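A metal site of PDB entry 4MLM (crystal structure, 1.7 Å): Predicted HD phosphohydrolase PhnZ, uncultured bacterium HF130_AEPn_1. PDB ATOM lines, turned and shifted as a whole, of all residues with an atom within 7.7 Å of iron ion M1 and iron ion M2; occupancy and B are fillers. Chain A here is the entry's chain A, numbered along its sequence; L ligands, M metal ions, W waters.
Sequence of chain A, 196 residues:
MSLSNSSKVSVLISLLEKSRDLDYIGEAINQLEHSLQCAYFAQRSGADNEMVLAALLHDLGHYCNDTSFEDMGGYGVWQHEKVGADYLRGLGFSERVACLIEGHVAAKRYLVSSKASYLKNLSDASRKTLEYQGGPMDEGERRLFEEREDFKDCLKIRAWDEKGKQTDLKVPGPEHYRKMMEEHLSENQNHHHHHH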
ATOM      1  N   TYR A  24      20.611   8.927  -8.179  1.00  0.00           N
ATOM      2  CA  TYR A  24      21.682   8.622  -7.241  1.00  0.00           C
ATOM      3  C   TYR A  24      21.677   9.657  -6.129  1.00  0.00           C
ATOM      4  O   TYR A  24      21.449   9.338  -4.960  1.00  0.00           O
ATOM      5  CB  TYR A  24      23.048   8.549  -7.928  1.00  0.00           C
ATOM      6  CG  TYR A  24      24.064   7.802  -7.097  1.00  0.00           C
ATOM      7  CD1 TYR A  24      24.143   6.420  -7.153  1.00  0.00           C
ATOM      8  CD2 TYR A  24      24.918   8.468  -6.229  1.00  0.00           C
ATOM      9  CE1 TYR A  24      25.064   5.706  -6.376  1.00  0.00           C
ATOM     10  CE2 TYR A  24      25.834   7.778  -5.451  1.00  0.00           C
ATOM     11  CZ  TYR A  24      25.922   6.407  -5.530  1.00  0.00           C
ATOM     12  OH  TYR A  24      26.838   5.718  -4.752  1.00  0.00           O
ATOM     13  N   GLN A  31      22.685   7.777 -11.601  1.00  0.00           N
ATOM     14  CA  GLN A  31      23.729   6.798 -11.309  1.00  0.00           C
ATOM     15  C   GLN A  31      24.836   6.794 -12.344  1.00  0.00           C
ATOM     16  O   GLN A  31      26.005   6.542 -12.015  1.00  0.00           O
ATOM     17  CB  GLN A  31      23.132   5.399 -11.167  1.00  0.00           C
ATOM     18  CG  GLN A  31      24.124   4.375 -10.651  1.00  0.00           C
ATOM     19  CD  GLN A  31      23.491   3.027 -10.450  1.00  0.00           C
ATOM     20  OE1 GLN A  31      22.641   2.867  -9.552  1.00  0.00           O
ATOM     21  NE2 GLN A  31      23.846   2.058 -11.288  1.00  0.00           N
ATOM     22  N   HIS A  34      27.094   9.703 -11.692  1.00  0.00           N
ATOM     23  CA  HIS A  34      27.875   9.370 -10.499  1.00  0.00           C
ATOM     24  C   HIS A  34      29.044   8.452 -10.834  1.00  0.00           C
ATOM     25  O   HIS A  34      30.178   8.697 -10.415  1.00  0.00           O
ATOM     26  CB  HIS A  34      26.968   8.695  -9.452  1.00  0.00           C
ATOM     27  CG  HIS A  34      27.717   7.963  -8.377  1.00  0.00           C
ATOM     28  ND1 HIS A  34      28.464   8.604  -7.413  1.00  0.00           N
ATOM     29  CD2 HIS A  34      27.794   6.636  -8.084  1.00  0.00           C
ATOM     30  CE1 HIS A  34      28.999   7.713  -6.603  1.00  0.00           C
ATOM     31  NE2 HIS A  34      28.604   6.514  -6.985  1.00  0.00           N
ATOM     32  N   SER A  35      28.757   7.410 -11.589  1.00  0.00           N
ATOM     33  CA  SER A  35      29.778   6.424 -11.939  1.00  0.00           C
ATOM     34  C   SER A  35      30.887   7.039 -12.771  1.00  0.00           C
ATOM     35  O   SER A  35      32.061   6.718 -12.589  1.00  0.00           O
ATOM     36  CB  SER A  35      29.147   5.254 -12.705  1.00  0.00           C
ATOM     37  OG  SER A  35      28.129   4.662 -11.918  1.00  0.00           O
ATOM     38  N   CYS A  38      33.162   9.164 -10.629  1.00  0.00           N
ATOM     39  CA  CYS A  38      34.080   8.316  -9.868  1.00  0.00           C
ATOM     40  C   CYS A  38      35.239   7.809 -10.716  1.00  0.00           C
ATOM     41  O   CYS A  38      36.379   7.819 -10.273  1.00  0.00           O
ATOM     42  CB  CYS A  38      33.344   7.127  -9.257  1.00  0.00           C
ATOM     43  SG  CYS A  38      32.197   7.613  -7.975  1.00  0.00           S
ATOM     44  N   ALA A  55      36.130   1.929 -10.170  1.00  0.00           N
ATOM     45  CA  ALA A  55      35.370   3.153  -9.888  1.00  0.00           C
ATOM     46  C   ALA A  55      34.208   3.320 -10.869  1.00  0.00           C
ATOM     47  O   ALA A  55      33.091   3.672 -10.475  1.00  0.00           O
ATOM     48  CB  ALA A  55      36.290   4.366  -9.927  1.00  0.00           C
ATOM     49  N   HIS A  58      31.465   0.328 -10.088  1.00  0.00           N
ATOM     50  CA  HIS A  58      31.183  -0.132  -8.724  1.00  0.00           C
ATOM     51  C   HIS A  58      29.689  -0.229  -8.391  1.00  0.00           C
ATOM     52  O   HIS A  58      29.305  -1.004  -7.507  1.00  0.00           O
ATOM     53  CB  HIS A  58      31.914   0.708  -7.663  1.00  0.00           C
ATOM     54  CG  HIS A  58      31.295   2.054  -7.410  1.00  0.00           C
ATOM     55  ND1 HIS A  58      31.497   3.127  -8.247  1.00  0.00           N
ATOM     56  CD2 HIS A  58      30.521   2.496  -6.395  1.00  0.00           C
ATOM     57  CE1 HIS A  58      30.849   4.178  -7.781  1.00  0.00           C
ATOM     58  NE2 HIS A  58      30.245   3.829  -6.654  1.00  0.00           N
ATOM     59  N   ASP A  59      28.860   0.537  -9.083  1.00  0.00           N
ATOM     60  CA  ASP A  59      27.435   0.561  -8.749  1.00  0.00           C
ATOM     61  C   ASP A  59      26.560  -0.103  -9.806  1.00  0.00           C
ATOM     62  O   ASP A  59      25.332  -0.017  -9.749  1.00  0.00           O
ATOM     63  CB  ASP A  59      26.969   2.008  -8.513  1.00  0.00           C
ATOM     64  CG  ASP A  59      27.276   2.477  -7.095  1.00  0.00           C
ATOM     65  OD1 ASP A  59      27.463   1.609  -6.201  1.00  0.00           O
ATOM     66  OD2 ASP A  59      27.317   3.715  -6.896  1.00  0.00           O
ATOM     67  N   LEU A  60      27.176  -0.791 -10.751  1.00  0.00           N
ATOM     68  CA  LEU A  60      26.417  -1.401 -11.838  1.00  0.00           C
ATOM     69  C   LEU A  60      25.358  -2.363 -11.302  1.00  0.00           C
ATOM     70  O   LEU A  60      24.301  -2.562 -11.918  1.00  0.00           O
ATOM     71  CB  LEU A  60      27.366  -2.127 -12.788  1.00  0.00           C
ATOM     72  CG  LEU A  60      26.817  -2.336 -14.201  1.00  0.00           C
ATOM     73  CD1 LEU A  60      26.504  -1.006 -14.857  1.00  0.00           C
ATOM     74  CD2 LEU A  60      27.792  -3.143 -15.039  1.00  0.00           C
ATOM     75  N   HIS A  62      23.145  -2.251  -8.933  1.00  0.00           N
ATOM     76  CA  HIS A  62      21.867  -1.787  -8.407  1.00  0.00           C
ATOM     77  C   HIS A  62      20.722  -2.209  -9.338  1.00  0.00           C
ATOM     78  O   HIS A  62      20.824  -2.083 -10.548  1.00  0.00           O
ATOM     79  CB  HIS A  62      21.834  -0.257  -8.289  1.00  0.00           C
ATOM     80  CG  HIS A  62      22.533   0.292  -7.072  1.00  0.00           C
ATOM     81  ND1 HIS A  62      22.196  -0.090  -5.791  1.00  0.00           N
ATOM     82  CD2 HIS A  62      23.497   1.225  -6.954  1.00  0.00           C
ATOM     83  CE1 HIS A  62      22.964   0.555  -4.933  1.00  0.00           C
ATOM     84  NE2 HIS A  62      23.757   1.379  -5.612  1.00  0.00           N
ATOM     85  N   HIS A  80      24.039  -4.849  -4.222  1.00  0.00           N
ATOM     86  CA  HIS A  80      24.604  -4.367  -5.483  1.00  0.00           C
ATOM     87  C   HIS A  80      26.086  -4.607  -5.617  1.00  0.00           C
ATOM     88  O   HIS A  80      26.571  -4.880  -6.720  1.00  0.00           O
ATOM     89  CB  HIS A  80      24.269  -2.891  -5.764  1.00  0.00           C
ATOM     90  CG  HIS A  80      25.066  -1.906  -4.939  1.00  0.00           C
ATOM     91  ND1 HIS A  80      24.946  -1.814  -3.575  1.00  0.00           N
ATOM     92  CD2 HIS A  80      25.949  -0.946  -5.304  1.00  0.00           C
ATOM     93  CE1 HIS A  80      25.738  -0.859  -3.131  1.00  0.00           C
ATOM     94  NE2 HIS A  80      26.357  -0.308  -4.156  1.00  0.00           N
ATOM     95  N   GLU A  81      26.826  -4.498  -4.509  1.00  0.00           N
ATOM     96  CA  GLU A  81      28.270  -4.712  -4.562  1.00  0.00           C
ATOM     97  C   GLU A  81      28.608  -6.155  -4.945  1.00  0.00           C
ATOM     98  O   GLU A  81      29.606  -6.412  -5.636  1.00  0.00           O
ATOM     99  CB  GLU A  81      28.957  -4.295  -3.255  1.00  0.00           C
ATOM    100  CG  GLU A  81      28.811  -5.258  -2.078  1.00  0.00           C
ATOM    101  CD  GLU A  81      27.485  -5.127  -1.340  1.00  0.00           C
ATOM    102  OE1 GLU A  81      26.552  -4.456  -1.843  1.00  0.00           O
ATOM    103  OE2 GLU A  81      27.377  -5.709  -0.233  1.00  0.00           O
ATOM    104  N   ILE A 101      35.238  -3.585  -6.024  1.00  0.00           N
ATOM    105  CA  ILE A 101      33.810  -3.290  -6.117  1.00  0.00           C
ATOM    106  C   ILE A 101      33.063  -3.926  -4.966  1.00  0.00           C
ATOM    107  O   ILE A 101      32.251  -3.275  -4.297  1.00  0.00           O
ATOM    108  CB  ILE A 101      33.236  -3.775  -7.464  1.00  0.00           C
ATOM    109  CG1 ILE A 101      33.812  -2.929  -8.597  1.00  0.00           C
ATOM    110  CG2 ILE A 101      31.690  -3.710  -7.463  1.00  0.00           C
ATOM    111  CD1 ILE A 101      33.368  -3.331 -10.003  1.00  0.00           C
ATOM    112  N   HIS A 104      33.291  -2.101  -1.441  1.00  0.00           N
ATOM    113  CA  HIS A 104      33.014  -0.667  -1.206  1.00  0.00           C
ATOM    114  C   HIS A 104      31.955  -0.408  -0.147  1.00  0.00           C
ATOM    115  O   HIS A 104      31.895   0.691   0.419  1.00  0.00           O
ATOM    116  CB  HIS A 104      32.769   0.135  -2.510  1.00  0.00           C
ATOM    117  CG  HIS A 104      31.362   0.118  -3.026  1.00  0.00           C
ATOM    118  ND1 HIS A 104      30.850  -0.906  -3.800  1.00  0.00           N
ATOM    119  CD2 HIS A 104      30.380   1.056  -2.965  1.00  0.00           C
ATOM    120  CE1 HIS A 104      29.611  -0.620  -4.156  1.00  0.00           C
ATOM    121  NE2 HIS A 104      29.294   0.568  -3.664  1.00  0.00           N
ATOM    122  N   VAL A 105      31.156  -1.414   0.186  1.00  0.00           N
ATOM    123  CA  VAL A 105      30.267  -1.290   1.330  1.00  0.00           C
ATOM    124  C   VAL A 105      31.062  -1.422   2.625  1.00  0.00           C
ATOM    125  O   VAL A 105      30.901  -0.615   3.551  1.00  0.00           O
ATOM    126  CB  VAL A 105      29.106  -2.290   1.295  1.00  0.00           C
ATOM    127  CG1 VAL A 105      28.412  -2.353   2.656  1.00  0.00           C
ATOM    128  CG2 VAL A 105      28.126  -1.877   0.195  1.00  0.00           C
ATOM    129  N   SER A 126      23.019   5.988   1.633  1.00  0.00           N
ATOM    130  CA  SER A 126      24.187   5.352   2.235  1.00  0.00           C
ATOM    131  C   SER A 126      24.091   5.322   3.759  1.00  0.00           C
ATOM    132  O   SER A 126      24.554   4.381   4.409  1.00  0.00           O
ATOM    133  CB  SER A 126      25.479   6.043   1.792  1.00  0.00           C
ATOM    134  OG  SER A 126      25.702   5.818   0.412  1.00  0.00           O
ATOM    135  N   GLN A 133      23.711  -3.205   7.208  1.00  0.00           N
ATOM    136  CA  GLN A 133      24.984  -3.770   6.773  1.00  0.00           C
ATOM    137  C   GLN A 133      25.865  -4.080   7.967  1.00  0.00           C
ATOM    138  O   GLN A 133      27.050  -4.387   7.820  1.00  0.00           O
ATOM    139  CB  GLN A 133      25.673  -2.790   5.830  1.00  0.00           C
ATOM    140  CG  GLN A 133      24.916  -2.582   4.535  1.00  0.00           C
ATOM    141  CD  GLN A 133      25.324  -1.327   3.781  1.00  0.00           C
ATOM    142  OE1 GLN A 133      25.893  -0.392   4.361  1.00  0.00           O
ATOM    143  NE2 GLN A 133      25.030  -1.281   2.488  1.00  0.00           N
ATOM    144  N   ILE A 157      38.480   4.046  -3.329  1.00  0.00           N
ATOM    145  CA  ILE A 157      37.250   3.845  -4.088  1.00  0.00           C
ATOM    146  C   ILE A 157      36.055   4.466  -3.365  1.00  0.00           C
ATOM    147  O   ILE A 157      35.215   5.114  -3.993  1.00  0.00           O
ATOM    148  CB  ILE A 157      36.969   2.328  -4.329  1.00  0.00           C
ATOM    149  CG1 ILE A 157      38.004   1.737  -5.290  1.00  0.00           C
ATOM    150  CG2 ILE A 157      35.545   2.115  -4.861  1.00  0.00           C
ATOM    151  CD1 ILE A 157      37.917   2.265  -6.688  1.00  0.00           C
ATOM    152  N   ARG A 158      35.974   4.278  -2.052  1.00  0.00           N
ATOM    153  CA  ARG A 158      34.811   4.789  -1.336  1.00  0.00           C
ATOM    154  C   ARG A 158      34.895   6.305  -1.113  1.00  0.00           C
ATOM    155  O   ARG A 158      33.879   7.003  -1.154  1.00  0.00           O
ATOM    156  CB  ARG A 158      34.585   4.037  -0.015  1.00  0.00           C
ATOM    157  CG  ARG A 158      33.297   4.467   0.706  1.00  0.00           C
ATOM    158  CD  ARG A 158      32.082   3.767   0.114  1.00  0.00           C
ATOM    159  NE  ARG A 158      30.852   4.546   0.293  1.00  0.00           N
ATOM    160  CZ  ARG A 158      29.637   4.041   0.150  1.00  0.00           C
ATOM    161  NH1 ARG A 158      29.505   2.745  -0.111  1.00  0.00           N
ATOM    162  NH2 ARG A 158      28.563   4.803   0.290  1.00  0.00           N
ATOM    163  N   TRP A 160      36.179   8.348  -3.278  1.00  0.00           N
ATOM    164  CA  TRP A 160      35.758   8.890  -4.574  1.00  0.00           C
ATOM    165  C   TRP A 160      34.244   8.758  -4.722  1.00  0.00           C
ATOM    166  O   TRP A 160      33.576   9.648  -5.209  1.00  0.00           O
ATOM    167  CB  TRP A 160      36.470   8.173  -5.728  1.00  0.00           C
ATOM    168  CG  TRP A 160      37.958   8.429  -5.730  1.00  0.00           C
ATOM    169  CD1 TRP A 160      38.606   9.561  -5.316  1.00  0.00           C
ATOM    170  CD2 TRP A 160      38.981   7.522  -6.175  1.00  0.00           C
ATOM    171  NE1 TRP A 160      39.964   9.405  -5.473  1.00  0.00           N
ATOM    172  CE2 TRP A 160      40.216   8.161  -6.002  1.00  0.00           C
ATOM    173  CE3 TRP A 160      38.967   6.227  -6.705  1.00  0.00           C
ATOM    174  CZ2 TRP A 160      41.431   7.557  -6.336  1.00  0.00           C
ATOM    175  CZ3 TRP A 160      40.162   5.631  -7.035  1.00  0.00           C
ATOM    176  CH2 TRP A 160      41.387   6.288  -6.849  1.00  0.00           C
ATOM    177  N   ASP A 161      33.725   7.627  -4.274  1.00  0.00           N
ATOM    178  CA  ASP A 161      32.289   7.378  -4.264  1.00  0.00           C
ATOM    179  C   ASP A 161      31.512   8.517  -3.607  1.00  0.00           C
ATOM    180  O   ASP A 161      30.580   9.071  -4.207  1.00  0.00           O
ATOM    181  CB  ASP A 161      32.070   6.052  -3.520  1.00  0.00           C
ATOM    182  CG  ASP A 161      30.686   5.514  -3.653  1.00  0.00           C
ATOM    183  OD1 ASP A 161      29.889   6.028  -4.460  1.00  0.00           O
ATOM    184  OD2 ASP A 161      30.396   4.533  -2.922  1.00  0.00           O
ATOM    185  N   GLU A 162      31.896   8.890  -2.387  1.00  0.00           N
ATOM    186  CA  GLU A 162      31.180   9.966  -1.694  1.00  0.00           C
ATOM    187  C   GLU A 162      31.347  11.300  -2.396  1.00  0.00           C
ATOM    188  O   GLU A 162      30.486  12.186  -2.281  1.00  0.00           O
ATOM    189  CB  GLU A 162      31.621  10.080  -0.236  1.00  0.00           C
ATOM    190  CG  GLU A 162      30.629   9.479   0.755  1.00  0.00           C
ATOM    191  CD  GLU A 162      30.431   7.990   0.543  1.00  0.00           C
ATOM    192  OE1 GLU A 162      31.357   7.214   0.844  1.00  0.00           O
ATOM    193  OE2 GLU A 162      29.333   7.584   0.061  1.00  0.00           O
ATOM    194  N   GLY A 164      31.448  11.649  -5.655  1.00  0.00           N
ATOM    195  CA  GLY A 164      30.822  11.604  -6.970  1.00  0.00           C
ATOM    196  C   GLY A 164      29.409  12.170  -7.020  1.00  0.00           C
ATOM    197  O   GLY A 164      28.461  11.481  -7.421  1.00  0.00           O
HETATM  198  O1  LIG L   1      24.224   4.093  -3.272  1.00  0.00           O
HETATM  199  O2  LIG L   1      25.577   2.703  -4.317  1.00  0.00           O
HETATM  200  C1  LIG L   1      25.190   3.282  -3.253  1.00  0.00           C
HETATM  201  C2  LIG L   1      25.877   2.986  -1.962  1.00  0.00           C
HETATM  202  O3  LIG L   1      26.886   2.051  -2.192  1.00  0.00           O
HETATM  203  C3  LIG L   1      24.853   2.480  -1.013  1.00  0.00           C
HETATM  204  O4  LIG L   1      24.140   1.442  -1.573  1.00  0.00           O
HETATM  205  C4  LIG L   1      25.552   1.992   0.200  1.00  0.00           C
HETATM  206  O5  LIG L   1      26.337   2.755   0.823  1.00  0.00           O
HETATM  207  O6  LIG L   1      25.350   0.821   0.585  1.00  0.00           O
HETATM  208 FE    FE M   1      27.425   1.635  -4.123  1.00  0.00          FE
HETATM  209 FE    FE M   2      28.580   4.841  -5.693  1.00  0.00          FE
HETATM  210  O   HOH W   1      28.467   3.567  -4.047  1.00  0.00           O
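The backbone carbonyl oxygen of Asp 59 lies within hydrogen-bond range of the side-chain amide nitrogen of Gln 31 (3.0 Å). SG of Cys 38 lies within hydrogen-bond range of O of His 34 (3.3 Å). ND1 of His 34 lies within hydrogen-bond range of O of Gly 164 (2.9 Å). OD2 of Asp 161 lies within salt-bridge range of NE of Arg 158 (3.2 Å). A ring nitrogen (ND1) of His 58 is in hydrogen-bond range of the backbone carbonyl oxygen (O) of Ala 55. The guanidinium group of Arg 158 lies close to the backbone carbonyl oxygen of His 104 (3.2 Å). A ring nitrogen (ND1) of His 104 is in hydrogen-bond range of the backbone carbonyl oxygen (O) of Ile 101 (2.8 Å). NE2 of His 62 lies close to NE2 of His 80, 3.4 Å away.
His 62 touches iron ion M1. Five residues have an atom within 4 Å of iron ion M1: His 58, Asp 59, His 62, His 80 and His 104. The nearest printed residue that does not touch iron ion M1 is Tyr 24 (4.2 Å).
Five residues have an atom within 4 Å of iron ion M2: Tyr 24, His 34, His 58, Asp 59 and Asp 161.
Iron ion M1 is bound by an oxygen (O3) of the ligand (2.0 Å), the side-chain carboxylate of Asp 59 (2.1 Å), an oxygen (O2) of the ligand (2.1 Å), water W1 (2.2 Å), a ring nitrogen (NE2) of His 104 (2.2 Å) and a ring nitrogen (NE2) of His 80 (2.2 Å).
Iron ion M2 is bound by the side-chain carboxylate of Asp 59 (2.1 Å), water W1 (2.1 Å), a ring nitrogen (NE2) of His 34 (2.1 Å), the side-chain carboxylate of Asp 161 (2.2 Å), the side-chain hydroxyl of Tyr 24 (2.2 Å) and a ring nitrogen (NE2) of His 58 (2.2 Å).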
